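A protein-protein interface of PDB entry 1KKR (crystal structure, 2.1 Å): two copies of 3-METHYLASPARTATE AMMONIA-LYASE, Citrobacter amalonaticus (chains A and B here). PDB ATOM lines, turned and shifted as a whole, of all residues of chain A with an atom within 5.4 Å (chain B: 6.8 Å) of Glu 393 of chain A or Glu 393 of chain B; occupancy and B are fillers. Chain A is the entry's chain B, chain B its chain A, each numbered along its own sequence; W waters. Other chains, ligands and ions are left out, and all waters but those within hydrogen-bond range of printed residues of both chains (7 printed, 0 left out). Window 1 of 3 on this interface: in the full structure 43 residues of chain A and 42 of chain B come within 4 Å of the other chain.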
ATOM      1  N   SER A  14     -14.068  20.248 -18.305  1.00  0.00           N
ATOM      2  CA  SER A  14     -14.983  19.114 -18.280  1.00  0.00           C
ATOM      3  C   SER A  14     -14.426  17.748 -18.720  1.00  0.00           C
ATOM      4  O   SER A  14     -15.194  16.845 -19.065  1.00  0.00           O
ATOM      5  CB  SER A  14     -16.211  19.503 -19.128  1.00  0.00           C
ATOM      6  OG  SER A  14     -17.051  20.428 -18.454  1.00  0.00           O
ATOM      7  N   PRO A 387     -18.995  21.052 -23.648  1.00  0.00           N
ATOM      8  CA  PRO A 387     -17.937  20.093 -23.429  1.00  0.00           C
ATOM      9  C   PRO A 387     -18.400  18.819 -22.840  1.00  0.00           C
ATOM     10  O   PRO A 387     -19.592  18.515 -22.831  1.00  0.00           O
ATOM     11  CB  PRO A 387     -17.071  20.821 -22.407  1.00  0.00           C
ATOM     12  CG  PRO A 387     -18.078  21.538 -21.573  1.00  0.00           C
ATOM     13  CD  PRO A 387     -19.155  21.951 -22.496  1.00  0.00           C
ATOM     14  N   GLY A 388     -17.428  18.073 -22.326  1.00  0.00           N
ATOM     15  CA  GLY A 388     -17.708  16.839 -21.628  1.00  0.00           C
ATOM     16  C   GLY A 388     -17.973  15.642 -22.493  1.00  0.00           C
ATOM     17  O   GLY A 388     -18.206  15.765 -23.704  1.00  0.00           O
ATOM     18  N   MET A 389     -17.947  14.469 -21.851  1.00  0.00           N
ATOM     19  CA  MET A 389     -18.207  13.204 -22.525  1.00  0.00           C
ATOM     20  C   MET A 389     -19.525  12.615 -22.085  1.00  0.00           C
ATOM     21  O   MET A 389     -19.832  11.498 -22.423  1.00  0.00           O
ATOM     22  CB  MET A 389     -17.058  12.231 -22.227  1.00  0.00           C
ATOM     23  CG  MET A 389     -15.745  12.540 -23.015  1.00  0.00           C
ATOM     24  SD  MET A 389     -16.061  12.547 -24.956  1.00  0.00           S
ATOM     25  CE  MET A 389     -16.847  11.569 -24.790  1.00  0.00           C
ATOM     26  N   GLY A 390     -20.301  13.347 -21.290  1.00  0.00           N
ATOM     27  CA  GLY A 390     -21.564  12.825 -20.829  1.00  0.00           C
ATOM     28  C   GLY A 390     -22.636  13.042 -21.873  1.00  0.00           C
ATOM     29  O   GLY A 390     -23.696  12.429 -21.835  1.00  0.00           O
ATOM     30  N   PHE A 391     -22.340  13.913 -22.819  1.00  0.00           N
ATOM     31  CA  PHE A 391     -23.276  14.320 -23.883  1.00  0.00           C
ATOM     32  C   PHE A 391     -24.476  15.175 -23.421  1.00  0.00           C
ATOM     33  O   PHE A 391     -24.662  16.254 -23.951  1.00  0.00           O
ATOM     34  CB  PHE A 391     -23.750  13.180 -24.820  1.00  0.00           C
ATOM     35  CG  PHE A 391     -24.914  13.593 -25.687  1.00  0.00           C
ATOM     36  CD1 PHE A 391     -26.210  13.218 -25.378  1.00  0.00           C
ATOM     37  CD2 PHE A 391     -24.729  14.469 -26.732  1.00  0.00           C
ATOM     38  CE1 PHE A 391     -27.279  13.649 -26.206  1.00  0.00           C
ATOM     39  CE2 PHE A 391     -25.787  14.923 -27.471  1.00  0.00           C
ATOM     40  CZ  PHE A 391     -27.038  14.516 -27.205  1.00  0.00           C
ATOM     41  N   ASP A 392     -25.279  14.703 -22.473  1.00  0.00           N
ATOM     42  CA  ASP A 392     -26.458  15.465 -22.022  1.00  0.00           C
ATOM     43  C   ASP A 392     -26.110  16.918 -21.630  1.00  0.00           C
ATOM     44  O   ASP A 392     -26.743  17.857 -22.070  1.00  0.00           O
ATOM     45  CB  ASP A 392     -27.108  14.746 -20.842  1.00  0.00           C
ATOM     46  CG  ASP A 392     -27.481  13.337 -21.190  1.00  0.00           C
ATOM     47  OD1 ASP A 392     -28.327  13.183 -22.114  1.00  0.00           O
ATOM     48  OD2 ASP A 392     -26.934  12.363 -20.631  1.00  0.00           O
ATOM     49  N   GLU A 393     -25.062  17.095 -20.844  1.00  0.00           N
ATOM     50  CA  GLU A 393     -24.693  18.411 -20.326  1.00  0.00           C
ATOM     51  C   GLU A 393     -24.316  19.361 -21.442  1.00  0.00           C
ATOM     52  O   GLU A 393     -24.766  20.506 -21.526  1.00  0.00           O
ATOM     53  CB  GLU A 393     -23.588  18.228 -19.301  1.00  0.00           C
ATOM     54  CG  GLU A 393     -24.047  17.336 -18.137  1.00  0.00           C
ATOM     55  CD  GLU A 393     -23.642  15.854 -18.241  1.00  0.00           C
ATOM     56  OE1 GLU A 393     -23.219  15.289 -17.172  1.00  0.00           O
ATOM     57  OE2 GLU A 393     -23.741  15.260 -19.355  1.00  0.00           O
ATOM     58  N   GLY A 394     -23.451  18.874 -22.310  1.00  0.00           N
ATOM     59  CA  GLY A 394     -23.138  19.579 -23.520  1.00  0.00           C
ATOM     60  C   GLY A 394     -24.272  19.985 -24.420  1.00  0.00           C
ATOM     61  O   GLY A 394     -24.277  21.073 -24.942  1.00  0.00           O
ATOM     62  N   LEU A 395     -25.226  19.109 -24.645  1.00  0.00           N
ATOM     63  CA  LEU A 395     -26.346  19.473 -25.458  1.00  0.00           C
ATOM     64  C   LEU A 395     -27.115  20.595 -24.766  1.00  0.00           C
ATOM     65  O   LEU A 395     -27.584  21.560 -25.393  1.00  0.00           O
ATOM     66  CB  LEU A 395     -27.261  18.254 -25.682  1.00  0.00           C
ATOM     67  CG  LEU A 395     -28.427  18.628 -26.620  1.00  0.00           C
ATOM     68  CD1 LEU A 395     -28.006  19.040 -28.049  1.00  0.00           C
ATOM     69  CD2 LEU A 395     -29.483  17.549 -26.712  1.00  0.00           C
ATOM     70  N   ASN A 396     -27.303  20.417 -23.471  1.00  0.00           N
ATOM     71  CA  ASN A 396     -28.034  21.387 -22.655  1.00  0.00           C
ATOM     72  C   ASN A 396     -27.369  22.756 -22.833  1.00  0.00           C
ATOM     73  O   ASN A 396     -28.023  23.723 -23.167  1.00  0.00           O
ATOM     74  CB  ASN A 396     -28.074  20.863 -21.212  1.00  0.00           C
ATOM     75  CG  ASN A 396     -28.723  21.819 -20.192  1.00  0.00           C
ATOM     76  OD1 ASN A 396     -29.004  23.029 -20.433  1.00  0.00           O
ATOM     77  ND2 ASN A 396     -28.937  21.259 -19.017  1.00  0.00           N
ATOM     78  N   ILE A 397     -26.051  22.793 -22.741  1.00  0.00           N
ATOM     79  CA  ILE A 397     -25.298  24.019 -22.869  1.00  0.00           C
ATOM     80  C   ILE A 397     -25.405  24.655 -24.232  1.00  0.00           C
ATOM     81  O   ILE A 397     -25.767  25.807 -24.346  1.00  0.00           O
ATOM     82  CB  ILE A 397     -23.816  23.785 -22.472  1.00  0.00           C
ATOM     83  CG1 ILE A 397     -23.740  23.570 -20.951  1.00  0.00           C
ATOM     84  CG2 ILE A 397     -22.976  24.960 -22.888  1.00  0.00           C
ATOM     85  CD1 ILE A 397     -22.472  22.925 -20.401  1.00  0.00           C
ATOM     86  N   VAL A 398     -25.143  23.866 -25.263  1.00  0.00           N
ATOM     87  CA  VAL A 398     -25.003  24.382 -26.583  1.00  0.00           C
ATOM     88  C   VAL A 398     -26.362  24.631 -27.184  1.00  0.00           C
ATOM     89  O   VAL A 398     -26.618  25.703 -27.704  1.00  0.00           O
ATOM     90  CB  VAL A 398     -24.190  23.402 -27.444  1.00  0.00           C
ATOM     91  CG1 VAL A 398     -24.235  23.790 -28.932  1.00  0.00           C
ATOM     92  CG2 VAL A 398     -22.743  23.352 -26.984  1.00  0.00           C
ATOM     93  N   SER B  13     -32.884  19.520 -20.811  1.00  0.00           N
ATOM     94  CA  SER B  13     -32.227  19.495 -19.503  1.00  0.00           C
ATOM     95  C   SER B  13     -31.093  18.476 -19.631  1.00  0.00           C
ATOM     96  O   SER B  13     -30.957  17.842 -20.694  1.00  0.00           O
ATOM     97  CB  SER B  13     -33.210  19.096 -18.423  1.00  0.00           C
ATOM     98  OG  SER B  13     -33.585  17.741 -18.502  1.00  0.00           O
ATOM     99  N   SER B  14     -30.284  18.341 -18.586  1.00  0.00           N
ATOM    100  CA  SER B  14     -29.075  17.500 -18.577  1.00  0.00           C
ATOM    101  C   SER B  14     -29.295  16.006 -18.234  1.00  0.00           C
ATOM    102  O   SER B  14     -28.337  15.284 -18.006  1.00  0.00           O
ATOM    103  CB  SER B  14     -27.949  18.133 -17.734  1.00  0.00           C
ATOM    104  OG  SER B  14     -27.340  19.287 -18.348  1.00  0.00           O
ATOM    105  N   PHE B  15     -30.536  15.534 -18.202  1.00  0.00           N
ATOM    106  CA  PHE B  15     -30.766  14.098 -18.092  1.00  0.00           C
ATOM    107  C   PHE B  15     -32.075  13.635 -18.718  1.00  0.00           C
ATOM    108  O   PHE B  15     -32.308  13.922 -19.872  1.00  0.00           O
ATOM    109  CB  PHE B  15     -30.503  13.536 -16.689  1.00  0.00           C
ATOM    110  CG  PHE B  15     -30.066  12.068 -16.702  1.00  0.00           C
ATOM    111  CD1 PHE B  15     -28.942  11.650 -17.387  1.00  0.00           C
ATOM    112  CD2 PHE B  15     -30.817  11.114 -16.054  1.00  0.00           C
ATOM    113  CE1 PHE B  15     -28.619  10.313 -17.435  1.00  0.00           C
ATOM    114  CE2 PHE B  15     -30.462   9.799 -16.063  1.00  0.00           C
ATOM    115  CZ  PHE B  15     -29.381   9.389 -16.747  1.00  0.00           C
ATOM    116  N   LYS B 183     -12.539   9.410 -11.226  1.00  0.00           N
ATOM    117  CA  LYS B 183     -12.755  10.787 -11.660  1.00  0.00           C
ATOM    118  C   LYS B 183     -12.818  11.701 -10.448  1.00  0.00           C
ATOM    119  O   LYS B 183     -12.144  12.734 -10.425  1.00  0.00           O
ATOM    120  CB  LYS B 183     -14.106  10.975 -12.436  1.00  0.00           C
ATOM    121  CG  LYS B 183     -14.141  10.578 -13.886  1.00  0.00           C
ATOM    122  CD  LYS B 183     -15.574  10.658 -14.415  1.00  0.00           C
ATOM    123  CE  LYS B 183     -15.634  10.404 -15.884  1.00  0.00           C
ATOM    124  NZ  LYS B 183     -16.991  10.684 -16.453  1.00  0.00           N
ATOM    125  N   LYS B 187     -10.150  14.773  -9.130  1.00  0.00           N
ATOM    126  CA  LYS B 187     -10.552  16.178  -9.064  1.00  0.00           C
ATOM    127  C   LYS B 187     -10.867  16.640  -7.636  1.00  0.00           C
ATOM    128  O   LYS B 187     -11.615  17.612  -7.423  1.00  0.00           O
ATOM    129  CB  LYS B 187     -11.732  16.426 -10.017  1.00  0.00           C
ATOM    130  CG  LYS B 187     -11.341  16.322 -11.504  1.00  0.00           C
ATOM    131  CD  LYS B 187     -12.522  16.425 -12.511  1.00  0.00           C
ATOM    132  CE  LYS B 187     -12.034  16.546 -13.960  1.00  0.00           C
ATOM    133  NZ  LYS B 187     -13.068  16.648 -15.036  1.00  0.00           N
ATOM    134  N   CYS B 361     -29.821  15.439 -11.365  1.00  0.00           N
ATOM    135  CA  CYS B 361     -29.045  15.350 -12.574  1.00  0.00           C
ATOM    136  C   CYS B 361     -29.852  15.927 -13.707  1.00  0.00           C
ATOM    137  O   CYS B 361     -29.299  16.280 -14.713  1.00  0.00           O
ATOM    138  CB  CYS B 361     -28.722  13.887 -12.934  1.00  0.00           C
ATOM    139  SG  CYS B 361     -30.176  12.789 -13.091  1.00  0.00           S
ATOM    140  N   GLU B 365     -27.482  23.853 -16.584  1.00  0.00           N
ATOM    141  CA  GLU B 365     -26.335  24.713 -16.270  1.00  0.00           C
ATOM    142  C   GLU B 365     -26.788  25.987 -15.557  1.00  0.00           C
ATOM    143  O   GLU B 365     -26.158  26.361 -14.585  1.00  0.00           O
ATOM    144  CB  GLU B 365     -25.406  25.010 -17.471  1.00  0.00           C
ATOM    145  CG  GLU B 365     -25.644  26.239 -18.337  1.00  0.00           C
ATOM    146  CD  GLU B 365     -26.923  26.231 -19.162  1.00  0.00           C
ATOM    147  OE1 GLU B 365     -27.916  25.504 -18.834  1.00  0.00           O
ATOM    148  OE2 GLU B 365     -26.926  27.027 -20.128  1.00  0.00           O
ATOM    149  N   ILE B 385     -23.178  18.456  -6.755  1.00  0.00           N
ATOM    150  CA  ILE B 385     -22.627  18.770  -8.042  1.00  0.00           C
ATOM    151  C   ILE B 385     -23.683  18.375  -9.096  1.00  0.00           C
ATOM    152  O   ILE B 385     -24.121  17.213  -9.194  1.00  0.00           O
ATOM    153  CB  ILE B 385     -21.284  18.039  -8.222  1.00  0.00           C
ATOM    154  CG1 ILE B 385     -20.308  18.645  -7.251  1.00  0.00           C
ATOM    155  CG2 ILE B 385     -20.698  18.205  -9.587  1.00  0.00           C
ATOM    156  CD1 ILE B 385     -19.083  17.797  -6.968  1.00  0.00           C
ATOM    157  N   LYS B 386     -24.037  19.322  -9.954  1.00  0.00           N
ATOM    158  CA  LYS B 386     -25.083  19.070 -10.928  1.00  0.00           C
ATOM    159  C   LYS B 386     -25.061  20.105 -12.013  1.00  0.00           C
ATOM    160  O   LYS B 386     -24.347  21.113 -11.921  1.00  0.00           O
ATOM    161  CB  LYS B 386     -26.426  19.173 -10.188  1.00  0.00           C
ATOM    162  CG  LYS B 386     -26.690  20.621  -9.647  1.00  0.00           C
ATOM    163  CD  LYS B 386     -27.904  20.739  -8.726  1.00  0.00           C
ATOM    164  CE  LYS B 386     -28.373  22.192  -8.493  1.00  0.00           C
ATOM    165  NZ  LYS B 386     -29.692  22.165  -7.736  1.00  0.00           N
ATOM    166  N   PRO B 387     -25.820  19.891 -13.081  1.00  0.00           N
ATOM    167  CA  PRO B 387     -26.647  18.727 -13.346  1.00  0.00           C
ATOM    168  C   PRO B 387     -25.817  17.677 -14.085  1.00  0.00           C
ATOM    169  O   PRO B 387     -24.604  17.824 -14.146  1.00  0.00           O
ATOM    170  CB  PRO B 387     -27.694  19.309 -14.309  1.00  0.00           C
ATOM    171  CG  PRO B 387     -26.900  20.283 -15.144  1.00  0.00           C
ATOM    172  CD  PRO B 387     -25.844  20.810 -14.215  1.00  0.00           C
ATOM    173  N   GLY B 388     -26.482  16.652 -14.627  1.00  0.00           N
ATOM    174  CA  GLY B 388     -25.877  15.639 -15.489  1.00  0.00           C
ATOM    175  C   GLY B 388     -25.391  14.410 -14.729  1.00  0.00           C
ATOM    176  O   GLY B 388     -25.249  14.417 -13.525  1.00  0.00           O
ATOM    177  N   MET B 389     -25.168  13.320 -15.444  1.00  0.00           N
ATOM    178  CA  MET B 389     -24.621  12.115 -14.809  1.00  0.00           C
ATOM    179  C   MET B 389     -23.169  11.876 -15.222  1.00  0.00           C
ATOM    180  O   MET B 389     -22.536  10.909 -14.744  1.00  0.00           O
ATOM    181  CB  MET B 389     -25.465  10.887 -15.072  1.00  0.00           C
ATOM    182  CG  MET B 389     -26.761  10.874 -14.290  1.00  0.00           C
ATOM    183  SD  MET B 389     -26.224  10.538 -12.447  1.00  0.00           S
ATOM    184  CE  MET B 389     -27.406  10.753 -11.856  1.00  0.00           C
ATOM    185  N   GLY B 390     -22.618  12.798 -16.013  1.00  0.00           N
ATOM    186  CA  GLY B 390     -21.228  12.732 -16.427  1.00  0.00           C
ATOM    187  C   GLY B 390     -20.257  13.114 -15.321  1.00  0.00           C
ATOM    188  O   GLY B 390     -19.094  12.720 -15.361  1.00  0.00           O
ATOM    189  N   PHE B 391     -20.759  13.819 -14.293  1.00  0.00           N
ATOM    190  CA  PHE B 391     -19.966  14.400 -13.186  1.00  0.00           C
ATOM    191  C   PHE B 391     -18.995  15.546 -13.581  1.00  0.00           C
ATOM    192  O   PHE B 391     -18.991  16.628 -12.968  1.00  0.00           O
ATOM    193  CB  PHE B 391     -19.214  13.333 -12.379  1.00  0.00           C
ATOM    194  CG  PHE B 391     -18.092  13.905 -11.545  1.00  0.00           C
ATOM    195  CD1 PHE B 391     -16.778  13.848 -11.988  1.00  0.00           C
ATOM    196  CD2 PHE B 391     -18.373  14.588 -10.391  1.00  0.00           C
ATOM    197  CE1 PHE B 391     -15.763  14.392 -11.235  1.00  0.00           C
ATOM    198  CE2 PHE B 391     -17.361  15.156  -9.638  1.00  0.00           C
ATOM    199  CZ  PHE B 391     -16.061  15.051 -10.057  1.00  0.00           C
ATOM    200  N   ASP B 392     -18.147  15.309 -14.559  1.00  0.00           N
ATOM    201  CA  ASP B 392     -17.159  16.329 -14.885  1.00  0.00           C
ATOM    202  C   ASP B 392     -17.816  17.676 -15.199  1.00  0.00           C
ATOM    203  O   ASP B 392     -17.355  18.716 -14.718  1.00  0.00           O
ATOM    204  CB  ASP B 392     -16.333  15.919 -16.097  1.00  0.00           C
ATOM    205  CG  ASP B 392     -15.657  14.575 -15.912  1.00  0.00           C
ATOM    206  OD1 ASP B 392     -14.751  14.488 -15.042  1.00  0.00           O
ATOM    207  OD2 ASP B 392     -16.001  13.574 -16.581  1.00  0.00           O
ATOM    208  N   GLU B 393     -18.827  17.646 -16.075  1.00  0.00           N
ATOM    209  CA  GLU B 393     -19.562  18.850 -16.476  1.00  0.00           C
ATOM    210  C   GLU B 393     -20.179  19.547 -15.269  1.00  0.00           C
ATOM    211  O   GLU B 393     -20.047  20.746 -15.124  1.00  0.00           O
ATOM    212  CB  GLU B 393     -20.592  18.524 -17.547  1.00  0.00           C
ATOM    213  CG  GLU B 393     -20.001  17.878 -18.823  1.00  0.00           C
ATOM    214  CD  GLU B 393     -20.037  16.337 -18.854  1.00  0.00           C
ATOM    215  OE1 GLU B 393     -20.310  15.756 -19.951  1.00  0.00           O
ATOM    216  OE2 GLU B 393     -19.745  15.713 -17.788  1.00  0.00           O
ATOM    217  N   GLY B 394     -20.873  18.794 -14.426  1.00  0.00           N
ATOM    218  CA  GLY B 394     -21.416  19.338 -13.181  1.00  0.00           C
ATOM    219  C   GLY B 394     -20.385  20.022 -12.307  1.00  0.00           C
ATOM    220  O   GLY B 394     -20.625  21.117 -11.754  1.00  0.00           O
ATOM    221  N   LEU B 395     -19.198  19.422 -12.224  1.00  0.00           N
ATOM    222  CA  LEU B 395     -18.189  19.981 -11.317  1.00  0.00           C
ATOM    223  C   LEU B 395     -17.690  21.305 -11.921  1.00  0.00           C
ATOM    224  O   LEU B 395     -17.551  22.368 -11.258  1.00  0.00           O
ATOM    225  CB  LEU B 395     -17.062  18.995 -11.074  1.00  0.00           C
ATOM    226  CG  LEU B 395     -15.981  19.605 -10.165  1.00  0.00           C
ATOM    227  CD1 LEU B 395     -16.470  19.639  -8.735  1.00  0.00           C
ATOM    228  CD2 LEU B 395     -14.677  18.851 -10.255  1.00  0.00           C
ATOM    229  N   ASN B 396     -17.432  21.230 -13.206  1.00  0.00           N
ATOM    230  CA  ASN B 396     -17.074  22.396 -13.951  1.00  0.00           C
ATOM    231  C   ASN B 396     -18.025  23.582 -13.726  1.00  0.00           C
ATOM    232  O   ASN B 396     -17.556  24.718 -13.424  1.00  0.00           O
ATOM    233  CB  ASN B 396     -17.032  22.017 -15.426  1.00  0.00           C
ATOM    234  CG  ASN B 396     -16.530  23.146 -16.321  1.00  0.00           C
ATOM    235  OD1 ASN B 396     -16.494  24.334 -15.944  1.00  0.00           O
ATOM    236  ND2 ASN B 396     -16.165  22.776 -17.521  1.00  0.00           N
ATOM    237  N   ILE B 397     -19.338  23.326 -13.885  1.00  0.00           N
ATOM    238  CA  ILE B 397     -20.416  24.305 -13.670  1.00  0.00           C
ATOM    239  C   ILE B 397     -20.460  24.837 -12.201  1.00  0.00           C
ATOM    240  O   ILE B 397     -20.368  26.044 -11.994  1.00  0.00           O
ATOM    241  CB  ILE B 397     -21.768  23.672 -14.044  1.00  0.00           C
ATOM    242  CG1 ILE B 397     -21.839  23.585 -15.557  1.00  0.00           C
ATOM    243  CG2 ILE B 397     -22.938  24.464 -13.526  1.00  0.00           C
ATOM    244  CD1 ILE B 397     -22.808  22.579 -15.999  1.00  0.00           C
ATOM    245  N   VAL B 398     -20.499  23.947 -11.198  1.00  0.00           N
ATOM    246  CA  VAL B 398     -20.698  24.348  -9.794  1.00  0.00           C
ATOM    247  C   VAL B 398     -19.421  24.894  -9.201  1.00  0.00           C
ATOM    248  O   VAL B 398     -19.393  26.016  -8.674  1.00  0.00           O
ATOM    249  CB  VAL B 398     -21.154  23.132  -8.971  1.00  0.00           C
ATOM    250  CG1 VAL B 398     -21.187  23.404  -7.483  1.00  0.00           C
ATOM    251  CG2 VAL B 398     -22.531  22.645  -9.495  1.00  0.00           C
HETATM  252  O   HOH W   1     -24.974  13.002 -18.470  1.00  0.00           O
HETATM  253  O   HOH W   2     -30.225  25.969 -20.200  1.00  0.00           O
HETATM  254  O   HOH W   3     -21.456  16.629 -22.203  1.00  0.00           O
HETATM  255  O   HOH W   4     -29.497  17.411 -22.868  1.00  0.00           O
HETATM  256  O   HOH W   5     -25.155  27.542 -22.176  1.00  0.00           O
HETATM  257  O   HOH W   6     -22.315  16.134 -14.750  1.00  0.00           O
HETATM  258  O   HOH W   7     -17.874  13.695 -18.810  1.00  0.00           O
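Water W4 bridges the backbone carbonyl oxygen (O) of Ser 13 of chain B and the backbone carbonyl oxygen (O) of Asp 392 of chain A. Water W3 lies within hydrogen-bond range of the side-chain carboxylate (OE1) of Glu 393 of chain B (2.7 Å), the backbone carbonyl oxygen (O) of Pro 387 of chain A (2.7 Å), the backbone NH (N) of Phe 391 of chain A (2.9 Å) and the backbone NH (N) of Gly 394 of chain A (3.0 Å). Water W1 lies within hydrogen-bond range of the side-chain carboxylate (OE2) of Glu 393 of chain A, the side-chain carboxylate (OD2) of Asp 392 of chain A, the backbone NH (N) of Met 389 of chain B and the backbone NH (N) of Gly 390 of chain B. Water W2 bridges the side-chain carboxylate (OE1) of Glu 365 of chain B (2.7 Å) and the side-chain amide oxygen (OD1) of Asn 396 of chain A (3.2 Å). Water W5 lies within hydrogen-bond range of the side-chain carboxylate of Glu 365 of chain B and the backbone carbonyl oxygen of Ile 397 of chain A. Water W7 lies within hydrogen-bond range of OD2 of Asp 392 of chain B (2.9 Å), OE2 of Glu 393 of chain B (2.9 Å), N of Met 389 of chain A (3.1 Å) and N of Gly 390 of chain A (3.5 Å).
Ser 14 of chain A touches Asp 392 of chain B, and with the chains exchanged Asp 392 of chain A touches Ser 14 of chain B. Ser 14 of chain A touches Glu 393 of chain B, and with the chains exchanged Glu 393 of chain A touches Ser 14 of chain B. Ser 14 of chain A touches Asn 396 of chain B, and with the chains exchanged Asn 396 of chain A touches Ser 14 of chain B. Gly 390 of chain A touches Glu 393 of chain B, and with the chains exchanged Glu 393 of chain A touches Gly 390 of chain B. 13 positions are printed for both chains.
O of Ser 14 of chain A touches CB of Asp 392 of chain B, at 3.3 Å. OG of Ser 14 of chain A touches CA of Glu 393 of chain B, at 3.6 Å. Gly 388 of chain A touches Glu 393 of chain B. Phe 391 of chain A touches Glu 393 of chain B. Asp 392 of chain A touches Ser 14 of chain B. CD1 of Phe 15 of chain B touches OD2 of Asp 392 of chain A (3.9 Å). Ser 14 of chain B touches Glu 393 of chain A. Gly 388 of chain B touches Glu 393 of chain A. Glu 393 of chain A touches Glu 393 of chain B (CB to CB, 3.5 Å). ND2 of Asn 396 of chain A touches C of Ser 13 of chain B (3.6 Å).
ND2 of Asn 396 of chain B sits at hydrogen-bond distance from OG of Ser 14 of chain A (2.7 Å). N of Met 389 of chain B is in hydrogen-bond range of OE1 of Glu 393 of chain A (3.3 Å). The side-chain carboxylate of Glu 365 of chain B sits close to the side-chain amide oxygen of Asn 396 of chain A, at 3.1 Å. The backbone NH of Gly 390 of chain A is in hydrogen-bond range of the side-chain carboxylate of Glu 393 of chain B, 2.8 Å away. The side-chain hydroxyl (OG) of Ser 14 of chain B is in hydrogen-bond range of the side-chain amide nitrogen (ND2) of Asn 396 of chain A (2.6 Å). The side-chain carboxylate (OE1) of Glu 393 of chain B is in hydrogen-bond range of the backbone NH (N) of Met 389 of chain A (3.3 Å). The backbone NH (N) of Gly 390 of chain B sits at hydrogen-bond distance from the side-chain carboxylate (OE1) of Glu 393 of chain A (2.8 Å).
The side-chain amino group (NZ) of Lys 187 of chain B is in salt-bridge range of the side-chain carboxylate (OD1) of Asp 392 of chain B (2.7 Å). NZ of Lys 183 of chain B sits at hydrogen-bond distance from O of Gly 390 of chain B (3.1 Å). OD2 of Asp 392 of chain B is in salt-bridge range of NZ of Lys 183 of chain B (3.1 Å). The backbone carbonyl oxygen (O) of Cys 361 of chain B lies within hydrogen-bond range of the backbone NH (N) of Gly 388 of chain B (2.8 Å).
Of the 21 printed residues of chain B, 10 touch a printed residue of chain A. Printed residues of chain B that touch a printed residue of chain A: Ser 13, Ser 14, Phe 15, Glu 365, Gly 388, Met 389, Gly 390, Asp 392, Glu 393 and Asn 396.
Printed residues of chain B within 4 Å of Met 389 of chain A: Glu 393 (3.3 Å). Glu 393 of chain A touches just these residues of chain B: Ser 14, Gly 388, Met 389, Gly 390 and Glu 393. Of the printed residues of chain B, Asn 396 of chain A touches Ser 13, Ser 14 and Glu 365. Pro 387 of chain B touches none of the printed residues of chain A. Printed residues of chain A within 4 Å of Gly 388 of chain B: Glu 393 (3.2 Å). Glu 393 of chain B touches six residues of chain A. Of the printed residues of chain A, Asn 396 of chain B touches Ser 14 (2.7 Å). The nearest residue of chain A that does not touch Glu 393 of chain B is Pro 387 of chain A (4.1 Å).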
